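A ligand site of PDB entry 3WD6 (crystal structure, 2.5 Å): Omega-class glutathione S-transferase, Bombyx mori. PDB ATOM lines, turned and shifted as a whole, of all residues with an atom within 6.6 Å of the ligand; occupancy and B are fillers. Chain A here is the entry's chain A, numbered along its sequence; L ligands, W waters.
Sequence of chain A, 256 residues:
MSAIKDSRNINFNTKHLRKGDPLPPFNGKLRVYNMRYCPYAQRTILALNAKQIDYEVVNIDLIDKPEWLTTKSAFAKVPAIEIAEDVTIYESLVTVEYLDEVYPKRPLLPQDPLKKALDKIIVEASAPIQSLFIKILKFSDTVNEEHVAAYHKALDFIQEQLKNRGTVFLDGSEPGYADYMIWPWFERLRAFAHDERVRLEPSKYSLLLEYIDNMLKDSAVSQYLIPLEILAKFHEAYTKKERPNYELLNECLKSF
Water W1 lies within hydrogen-bond range of O of Pro 79 (2.7 Å), O1 of the ligand (2.8 Å), N of Glu 91 (3.1 Å) and O of Val 78 (3.3 Å).
Water W2 lies within hydrogen-bond range of O2 of the ligand, N of Leu 93 and OG of Ser 92.
Tyr 40 touches the ligand.
O of Leu 62 touches O5 of the ligand, at 3.6 Å.
Ala 76 touches the ligand.
Lys 77 touches the ligand.
Pro 79 touches the ligand.
The guanidinium group (NH1) of Arg 43 is in hydrogen-bond range of the side-chain hydroxyl (OG) of Ser 92, at 3.0 Å.
The backbone carbonyl oxygen (O) of Ser 92 is in hydrogen-bond range of the side-chain hydroxyl (OG1) of Thr 95 (2.7 Å).
The side-chain sulfur (SG) of Cys 38 lies close to the backbone NH (N) of Tyr 40 (3.4 Å).
The side-chain sulfur (SD) of Met 35 lies close to the backbone NH (N) of Cys 38.
The side-chain sulfur (SG) of Cys 38 sits at hydrogen-bond distance from the backbone NH (N) of Ala 41, 3.3 Å away.
The backbone carbonyl oxygen (O) of Ala 76 sits at hydrogen-bond distance from the side-chain amino group (NZ) of Lys 65, at 2.7 Å.
OH of Tyr 246 is in hydrogen-bond range of N of Leu 62 (3.3 Å).
The backbone NH (N) of Ser 92 sits at hydrogen-bond distance from an oxygen (O1) of the ligand, 2.7 Å away.
The side-chain hydroxyl (OG) of Ser 92 lies within hydrogen-bond range of an oxygen (O2) of the ligand (2.6 Å).
A sulfur (S1) of the ligand lies close to the side-chain sulfur of Cys 38 (2.8 Å).
OE1 of Glu 91 is in salt-bridge range of N1 of the ligand, at 2.8 Å.
O4 of the ligand lies within hydrogen-bond range of N of Val 78 (3.0 Å).
A nitrogen (N2) of the ligand lies within hydrogen-bond range of the backbone carbonyl oxygen (O) of Val 78 (2.9 Å).
O6 of the ligand is in salt-bridge range of NZ of Lys 65 (3.1 Å).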
ATOM      1  N   MET A  35     -14.766 -12.982  27.894  1.00  0.00           N
ATOM      2  CA  MET A  35     -14.024 -11.771  28.250  1.00  0.00           C
ATOM      3  C   MET A  35     -13.343 -11.205  27.004  1.00  0.00           C
ATOM      4  O   MET A  35     -12.766 -11.951  26.207  1.00  0.00           O
ATOM      5  CB  MET A  35     -13.104 -11.930  29.452  1.00  0.00           C
ATOM      6  CG  MET A  35     -11.700 -12.248  29.150  1.00  0.00           C
ATOM      7  SD  MET A  35     -10.587 -10.809  28.971  1.00  0.00           S
ATOM      8  CE  MET A  35      -9.044 -11.746  29.047  1.00  0.00           C
ATOM      9  N   TYR A  37     -10.912  -9.812  25.737  1.00  0.00           N
ATOM     10  CA  TYR A  37      -9.556  -9.999  25.260  1.00  0.00           C
ATOM     11  C   TYR A  37      -9.199 -11.478  25.254  1.00  0.00           C
ATOM     12  O   TYR A  37      -8.069 -11.845  24.922  1.00  0.00           O
ATOM     13  CB  TYR A  37      -8.594  -9.168  26.150  1.00  0.00           C
ATOM     14  CG  TYR A  37      -9.006  -7.709  26.182  1.00  0.00           C
ATOM     15  CD1 TYR A  37      -8.511  -6.803  25.251  1.00  0.00           C
ATOM     16  CD2 TYR A  37      -9.940  -7.267  27.101  1.00  0.00           C
ATOM     17  CE1 TYR A  37      -8.930  -5.466  25.267  1.00  0.00           C
ATOM     18  CE2 TYR A  37     -10.358  -5.950  27.125  1.00  0.00           C
ATOM     19  CZ  TYR A  37      -9.868  -5.057  26.199  1.00  0.00           C
ATOM     20  OH  TYR A  37     -10.305  -3.739  26.254  1.00  0.00           O
ATOM     21  N   CYS A  38     -10.160 -12.327  25.614  1.00  0.00           N
ATOM     22  CA  CYS A  38      -9.889 -13.756  25.583  1.00  0.00           C
ATOM     23  C   CYS A  38      -9.920 -14.343  24.155  1.00  0.00           C
ATOM     24  O   CYS A  38     -10.980 -14.369  23.505  1.00  0.00           O
ATOM     25  CB  CYS A  38     -10.828 -14.529  26.508  1.00  0.00           C
ATOM     26  SG  CYS A  38     -10.506 -16.331  26.436  1.00  0.00           S
ATOM     27  N   PRO A  39      -8.773 -14.835  23.658  1.00  0.00           N
ATOM     28  CA  PRO A  39      -8.827 -15.384  22.288  1.00  0.00           C
ATOM     29  C   PRO A  39      -9.706 -16.623  22.217  1.00  0.00           C
ATOM     30  O   PRO A  39     -10.341 -16.840  21.163  1.00  0.00           O
ATOM     31  CB  PRO A  39      -7.375 -15.739  21.950  1.00  0.00           C
ATOM     32  CG  PRO A  39      -6.703 -15.911  23.282  1.00  0.00           C
ATOM     33  CD  PRO A  39      -7.422 -14.948  24.253  1.00  0.00           C
ATOM     34  N   TYR A  40      -9.732 -17.429  23.288  1.00  0.00           N
ATOM     35  CA  TYR A  40     -10.523 -18.653  23.248  1.00  0.00           C
ATOM     36  C   TYR A  40     -11.999 -18.316  23.127  1.00  0.00           C
ATOM     37  O   TYR A  40     -12.715 -18.904  22.294  1.00  0.00           O
ATOM     38  CB  TYR A  40     -10.242 -19.548  24.471  1.00  0.00           C
ATOM     39  CG  TYR A  40      -8.867 -20.133  24.415  1.00  0.00           C
ATOM     40  CD1 TYR A  40      -8.574 -21.219  23.587  1.00  0.00           C
ATOM     41  CD2 TYR A  40      -7.824 -19.567  25.159  1.00  0.00           C
ATOM     42  CE1 TYR A  40      -7.300 -21.743  23.523  1.00  0.00           C
ATOM     43  CE2 TYR A  40      -6.537 -20.094  25.096  1.00  0.00           C
ATOM     44  CZ  TYR A  40      -6.275 -21.183  24.278  1.00  0.00           C
ATOM     45  OH  TYR A  40      -5.002 -21.686  24.205  1.00  0.00           O
ATOM     46  N   ALA A  41     -12.451 -17.372  23.927  1.00  0.00           N
ATOM     47  CA  ALA A  41     -13.835 -16.917  23.840  1.00  0.00           C
ATOM     48  C   ALA A  41     -14.107 -16.279  22.473  1.00  0.00           C
ATOM     49  O   ALA A  41     -15.242 -16.359  21.970  1.00  0.00           O
ATOM     50  CB  ALA A  41     -14.131 -15.960  24.969  1.00  0.00           C
ATOM     51  N   ARG A  43     -13.253 -17.301  19.590  1.00  0.00           N
ATOM     52  CA  ARG A  43     -13.711 -18.378  18.712  1.00  0.00           C
ATOM     53  C   ARG A  43     -15.221 -18.472  18.699  1.00  0.00           C
ATOM     54  O   ARG A  43     -15.834 -18.646  17.629  1.00  0.00           O
ATOM     55  CB  ARG A  43     -13.139 -19.720  19.183  1.00  0.00           C
ATOM     56  CG  ARG A  43     -11.683 -19.896  18.880  1.00  0.00           C
ATOM     57  CD  ARG A  43     -11.158 -21.069  19.626  1.00  0.00           C
ATOM     58  NE  ARG A  43      -9.917 -21.565  19.051  1.00  0.00           N
ATOM     59  CZ  ARG A  43      -9.227 -22.582  19.538  1.00  0.00           C
ATOM     60  NH1 ARG A  43      -9.661 -23.205  20.639  1.00  0.00           N
ATOM     61  NH2 ARG A  43      -8.114 -22.981  18.905  1.00  0.00           N
ATOM     62  N   LEU A  62     -11.768 -11.888  35.106  1.00  0.00           N
ATOM     63  CA  LEU A  62     -11.126 -13.179  35.377  1.00  0.00           C
ATOM     64  C   LEU A  62     -10.126 -13.115  36.527  1.00  0.00           C
ATOM     65  O   LEU A  62      -9.487 -14.121  36.855  1.00  0.00           O
ATOM     66  CB  LEU A  62     -10.395 -13.669  34.141  1.00  0.00           C
ATOM     67  CG  LEU A  62     -11.250 -14.031  32.937  1.00  0.00           C
ATOM     68  CD1 LEU A  62     -10.349 -14.529  31.823  1.00  0.00           C
ATOM     69  CD2 LEU A  62     -12.291 -15.088  33.322  1.00  0.00           C
ATOM     70  N   ILE A  63      -9.969 -11.941  37.098  1.00  0.00           N
ATOM     71  CA  ILE A  63      -9.053 -11.745  38.211  1.00  0.00           C
ATOM     72  C   ILE A  63      -9.876 -11.881  39.468  1.00  0.00           C
ATOM     73  O   ILE A  63      -9.466 -12.528  40.437  1.00  0.00           O
ATOM     74  CB  ILE A  63      -8.405 -10.338  38.156  1.00  0.00           C
ATOM     75  CG1 ILE A  63      -7.404 -10.257  36.987  1.00  0.00           C
ATOM     76  CG2 ILE A  63      -7.726  -9.997  39.488  1.00  0.00           C
ATOM     77  CD1 ILE A  63      -6.245 -11.207  37.119  1.00  0.00           C
ATOM     78  N   LYS A  65     -13.341 -13.173  39.862  1.00  0.00           N
ATOM     79  CA  LYS A  65     -14.458 -13.873  39.222  1.00  0.00           C
ATOM     80  C   LYS A  65     -15.739 -13.766  40.007  1.00  0.00           C
ATOM     81  O   LYS A  65     -15.727 -13.828  41.254  1.00  0.00           O
ATOM     82  CB  LYS A  65     -14.132 -15.354  39.000  1.00  0.00           C
ATOM     83  CG  LYS A  65     -13.114 -15.611  37.914  1.00  0.00           C
ATOM     84  CD  LYS A  65     -12.812 -17.112  37.763  1.00  0.00           C
ATOM     85  CE  LYS A  65     -11.523 -17.305  36.970  1.00  0.00           C
ATOM     86  NZ  LYS A  65     -11.098 -18.734  36.905  1.00  0.00           N
ATOM     87  N   PHE A  75     -15.146 -25.231  34.757  1.00  0.00           N
ATOM     88  CA  PHE A  75     -13.708 -25.050  34.979  1.00  0.00           C
ATOM     89  C   PHE A  75     -13.329 -23.606  35.304  1.00  0.00           C
ATOM     90  O   PHE A  75     -12.144 -23.249  35.276  1.00  0.00           O
ATOM     91  CB  PHE A  75     -12.903 -25.521  33.772  1.00  0.00           C
ATOM     92  CG  PHE A  75     -13.279 -26.885  33.285  1.00  0.00           C
ATOM     93  CD1 PHE A  75     -13.819 -27.829  34.163  1.00  0.00           C
ATOM     94  CD2 PHE A  75     -13.106 -27.232  31.934  1.00  0.00           C
ATOM     95  CE1 PHE A  75     -14.174 -29.091  33.712  1.00  0.00           C
ATOM     96  CE2 PHE A  75     -13.461 -28.498  31.474  1.00  0.00           C
ATOM     97  CZ  PHE A  75     -13.997 -29.421  32.366  1.00  0.00           C
ATOM     98  N   ALA A  76     -14.328 -22.788  35.645  1.00  0.00           N
ATOM     99  CA  ALA A  76     -14.110 -21.353  35.855  1.00  0.00           C
ATOM    100  C   ALA A  76     -13.384 -20.656  34.678  1.00  0.00           C
ATOM    101  O   ALA A  76     -12.612 -19.725  34.867  1.00  0.00           O
ATOM    102  CB  ALA A  76     -13.391 -21.088  37.187  1.00  0.00           C
ATOM    103  N   LYS A  77     -13.688 -21.096  33.465  1.00  0.00           N
ATOM    104  CA  LYS A  77     -13.091 -20.507  32.269  1.00  0.00           C
ATOM    105  C   LYS A  77     -14.126 -19.864  31.360  1.00  0.00           C
ATOM    106  O   LYS A  77     -15.347 -20.125  31.487  1.00  0.00           O
ATOM    107  CB  LYS A  77     -12.312 -21.554  31.477  1.00  0.00           C
ATOM    108  CG  LYS A  77     -10.978 -21.911  32.105  1.00  0.00           C
ATOM    109  CD  LYS A  77     -10.402 -23.178  31.476  1.00  0.00           C
ATOM    110  CE  LYS A  77      -9.163 -23.621  32.230  1.00  0.00           C
ATOM    111  NZ  LYS A  77      -8.631 -24.911  31.694  1.00  0.00           N
ATOM    112  N   VAL A  78     -13.644 -19.017  30.452  1.00  0.00           N
ATOM    113  CA  VAL A  78     -14.441 -18.551  29.306  1.00  0.00           C
ATOM    114  C   VAL A  78     -13.825 -19.136  28.036  1.00  0.00           C
ATOM    115  O   VAL A  78     -12.618 -19.432  28.015  1.00  0.00           O
ATOM    116  CB  VAL A  78     -14.474 -17.007  29.197  1.00  0.00           C
ATOM    117  CG1 VAL A  78     -15.361 -16.409  30.294  1.00  0.00           C
ATOM    118  CG2 VAL A  78     -13.056 -16.436  29.260  1.00  0.00           C
ATOM    119  N   PRO A  79     -14.627 -19.316  26.978  1.00  0.00           N
ATOM    120  CA  PRO A  79     -16.065 -19.008  26.937  1.00  0.00           C
ATOM    121  C   PRO A  79     -16.943 -20.127  27.530  1.00  0.00           C
ATOM    122  O   PRO A  79     -16.524 -21.295  27.727  1.00  0.00           O
ATOM    123  CB  PRO A  79     -16.351 -18.975  25.425  1.00  0.00           C
ATOM    124  CG  PRO A  79     -15.418 -20.097  24.879  1.00  0.00           C
ATOM    125  CD  PRO A  79     -14.136 -19.920  25.719  1.00  0.00           C
ATOM    126  N   TYR A  90     -19.257 -25.360  27.637  1.00  0.00           N
ATOM    127  CA  TYR A  90     -18.009 -24.614  27.704  1.00  0.00           C
ATOM    128  C   TYR A  90     -16.911 -25.395  27.008  1.00  0.00           C
ATOM    129  O   TYR A  90     -17.156 -26.521  26.552  1.00  0.00           O
ATOM    130  CB  TYR A  90     -17.621 -24.275  29.136  1.00  0.00           C
ATOM    131  CG  TYR A  90     -17.910 -25.390  30.110  1.00  0.00           C
ATOM    132  CD1 TYR A  90     -19.176 -25.552  30.659  1.00  0.00           C
ATOM    133  CD2 TYR A  90     -16.916 -26.282  30.480  1.00  0.00           C
ATOM    134  CE1 TYR A  90     -19.444 -26.577  31.555  1.00  0.00           C
ATOM    135  CE2 TYR A  90     -17.169 -27.314  31.368  1.00  0.00           C
ATOM    136  CZ  TYR A  90     -18.441 -27.448  31.905  1.00  0.00           C
ATOM    137  OH  TYR A  90     -18.685 -28.479  32.783  1.00  0.00           O
ATOM    138  N   GLU A  91     -15.727 -24.804  26.950  1.00  0.00           N
ATOM    139  CA  GLU A  91     -14.641 -25.265  26.070  1.00  0.00           C
ATOM    140  C   GLU A  91     -14.918 -24.760  24.659  1.00  0.00           C
ATOM    141  O   GLU A  91     -15.863 -25.210  23.994  1.00  0.00           O
ATOM    142  CB  GLU A  91     -14.462 -26.790  26.083  1.00  0.00           C
ATOM    143  CG  GLU A  91     -13.871 -27.296  27.384  1.00  0.00           C
ATOM    144  CD  GLU A  91     -12.473 -26.745  27.626  1.00  0.00           C
ATOM    145  OE1 GLU A  91     -11.602 -26.905  26.729  1.00  0.00           O
ATOM    146  OE2 GLU A  91     -12.257 -26.153  28.707  1.00  0.00           O
ATOM    147  N   SER A  92     -14.108 -23.794  24.232  1.00  0.00           N
ATOM    148  CA  SER A  92     -14.371 -23.018  23.026  1.00  0.00           C
ATOM    149  C   SER A  92     -14.694 -23.880  21.809  1.00  0.00           C
ATOM    150  O   SER A  92     -15.685 -23.615  21.111  1.00  0.00           O
ATOM    151  CB  SER A  92     -13.188 -22.095  22.736  1.00  0.00           C
ATOM    152  OG  SER A  92     -12.031 -22.841  22.408  1.00  0.00           O
ATOM    153  N   LEU A  93     -13.872 -24.903  21.551  1.00  0.00           N
ATOM    154  CA  LEU A  93     -14.086 -25.762  20.394  1.00  0.00           C
ATOM    155  C   LEU A  93     -15.338 -26.630  20.560  1.00  0.00           C
ATOM    156  O   LEU A  93     -15.981 -27.009  19.571  1.00  0.00           O
ATOM    157  CB  LEU A  93     -12.872 -26.646  20.125  1.00  0.00           C
ATOM    158  CG  LEU A  93     -11.601 -25.918  19.672  1.00  0.00           C
ATOM    159  CD1 LEU A  93     -10.495 -26.920  19.336  1.00  0.00           C
ATOM    160  CD2 LEU A  93     -11.901 -25.008  18.452  1.00  0.00           C
ATOM    161  N   VAL A  94     -15.683 -26.926  21.804  1.00  0.00           N
ATOM    162  CA  VAL A  94     -16.903 -27.677  22.054  1.00  0.00           C
ATOM    163  C   VAL A  94     -18.117 -26.814  21.715  1.00  0.00           C
ATOM    164  O   VAL A  94     -19.086 -27.290  21.102  1.00  0.00           O
ATOM    165  CB  VAL A  94     -16.973 -28.163  23.489  1.00  0.00           C
ATOM    166  CG1 VAL A  94     -18.326 -28.803  23.772  1.00  0.00           C
ATOM    167  CG2 VAL A  94     -15.840 -29.155  23.756  1.00  0.00           C
ATOM    168  N   THR A  95     -18.060 -25.544  22.101  1.00  0.00           N
ATOM    169  CA  THR A  95     -19.168 -24.641  21.850  1.00  0.00           C
ATOM    170  C   THR A  95     -19.365 -24.424  20.355  1.00  0.00           C
ATOM    171  O   THR A  95     -20.482 -24.477  19.832  1.00  0.00           O
ATOM    172  CB  THR A  95     -18.975 -23.301  22.551  1.00  0.00           C
ATOM    173  OG1 THR A  95     -18.003 -22.534  21.825  1.00  0.00           O
ATOM    174  CG2 THR A  95     -18.491 -23.563  23.984  1.00  0.00           C
ATOM    175  N   LYS A 138       3.336 -13.454  29.408  1.00  0.00           N
ATOM    176  CA  LYS A 138       3.305 -13.656  30.871  1.00  0.00           C
ATOM    177  C   LYS A 138       4.566 -14.266  31.499  1.00  0.00           C
ATOM    178  O   LYS A 138       4.727 -14.229  32.716  1.00  0.00           O
ATOM    179  CB  LYS A 138       2.095 -14.511  31.293  1.00  0.00           C
ATOM    180  CG  LYS A 138       0.734 -13.893  31.012  1.00  0.00           C
ATOM    181  CD  LYS A 138      -0.335 -14.505  31.939  1.00  0.00           C
ATOM    182  CE  LYS A 138      -1.752 -14.217  31.432  1.00  0.00           C
ATOM    183  NZ  LYS A 138      -2.807 -14.850  32.293  1.00  0.00           N
ATOM    184  N   TYR A 246     -10.071  -4.282  32.152  1.00  0.00           N
ATOM    185  CA  TYR A 246     -10.986  -4.913  31.204  1.00  0.00           C
ATOM    186  C   TYR A 246     -11.929  -3.898  30.540  1.00  0.00           C
ATOM    187  O   TYR A 246     -12.754  -4.287  29.739  1.00  0.00           O
ATOM    188  CB  TYR A 246     -11.835  -5.968  31.903  1.00  0.00           C
ATOM    189  CG  TYR A 246     -11.067  -7.163  32.446  1.00  0.00           C
ATOM    190  CD1 TYR A 246     -10.316  -7.973  31.611  1.00  0.00           C
ATOM    191  CD2 TYR A 246     -11.118  -7.489  33.796  1.00  0.00           C
ATOM    192  CE1 TYR A 246      -9.613  -9.076  32.112  1.00  0.00           C
ATOM    193  CE2 TYR A 246     -10.429  -8.585  34.305  1.00  0.00           C
ATOM    194  CZ  TYR A 246      -9.679  -9.374  33.461  1.00  0.00           C
ATOM    195  OH  TYR A 246      -8.997 -10.482  33.952  1.00  0.00           O
HETATM  196  N1  LIG L   1      -9.531 -24.964  26.645  1.00  0.00           N
HETATM  197  C1  LIG L   1     -10.371 -23.801  26.964  1.00  0.00           C
HETATM  198  C2  LIG L   1     -11.206 -23.344  25.765  1.00  0.00           C
HETATM  199  O1  LIG L   1     -12.339 -22.755  25.931  1.00  0.00           O
HETATM  200  O2  LIG L   1     -10.771 -23.598  24.587  1.00  0.00           O
HETATM  201  C3  LIG L   1      -9.479 -22.679  27.484  1.00  0.00           C
HETATM  202  C4  LIG L   1     -10.069 -21.323  27.632  1.00  0.00           C
HETATM  203  C5  LIG L   1      -9.283 -20.360  28.491  1.00  0.00           C
HETATM  204  O3  LIG L   1      -8.107 -20.574  28.781  1.00  0.00           O
HETATM  205  N2  LIG L   1      -9.899 -19.181  29.001  1.00  0.00           N
HETATM  206  C6  LIG L   1      -9.090 -18.307  29.854  1.00  0.00           C
HETATM  207  C7  LIG L   1      -9.681 -18.346  31.249  1.00  0.00           C
HETATM  208  O4  LIG L   1     -10.898 -18.308  31.374  1.00  0.00           O
HETATM  209  C8  LIG L   1      -9.152 -16.906  29.348  1.00  0.00           C
HETATM  210  S1  LIG L   1      -8.158 -16.483  27.952  1.00  0.00           S
HETATM  211  N3  LIG L   1      -8.813 -18.420  32.403  1.00  0.00           N
HETATM  212  C9  LIG L   1      -9.394 -18.449  33.751  1.00  0.00           C
HETATM  213  C10 LIG L   1      -8.543 -17.900  34.825  1.00  0.00           C
HETATM  214  O5  LIG L   1      -8.177 -16.694  34.770  1.00  0.00           O
HETATM  215  O6  LIG L   1      -8.219 -18.620  35.796  1.00  0.00           O
HETATM  216  O   HOH W   1     -14.091 -22.413  28.040  1.00  0.00           O
HETATM  217  O   HOH W   2     -11.407 -25.981  23.146  1.00  0.00           O
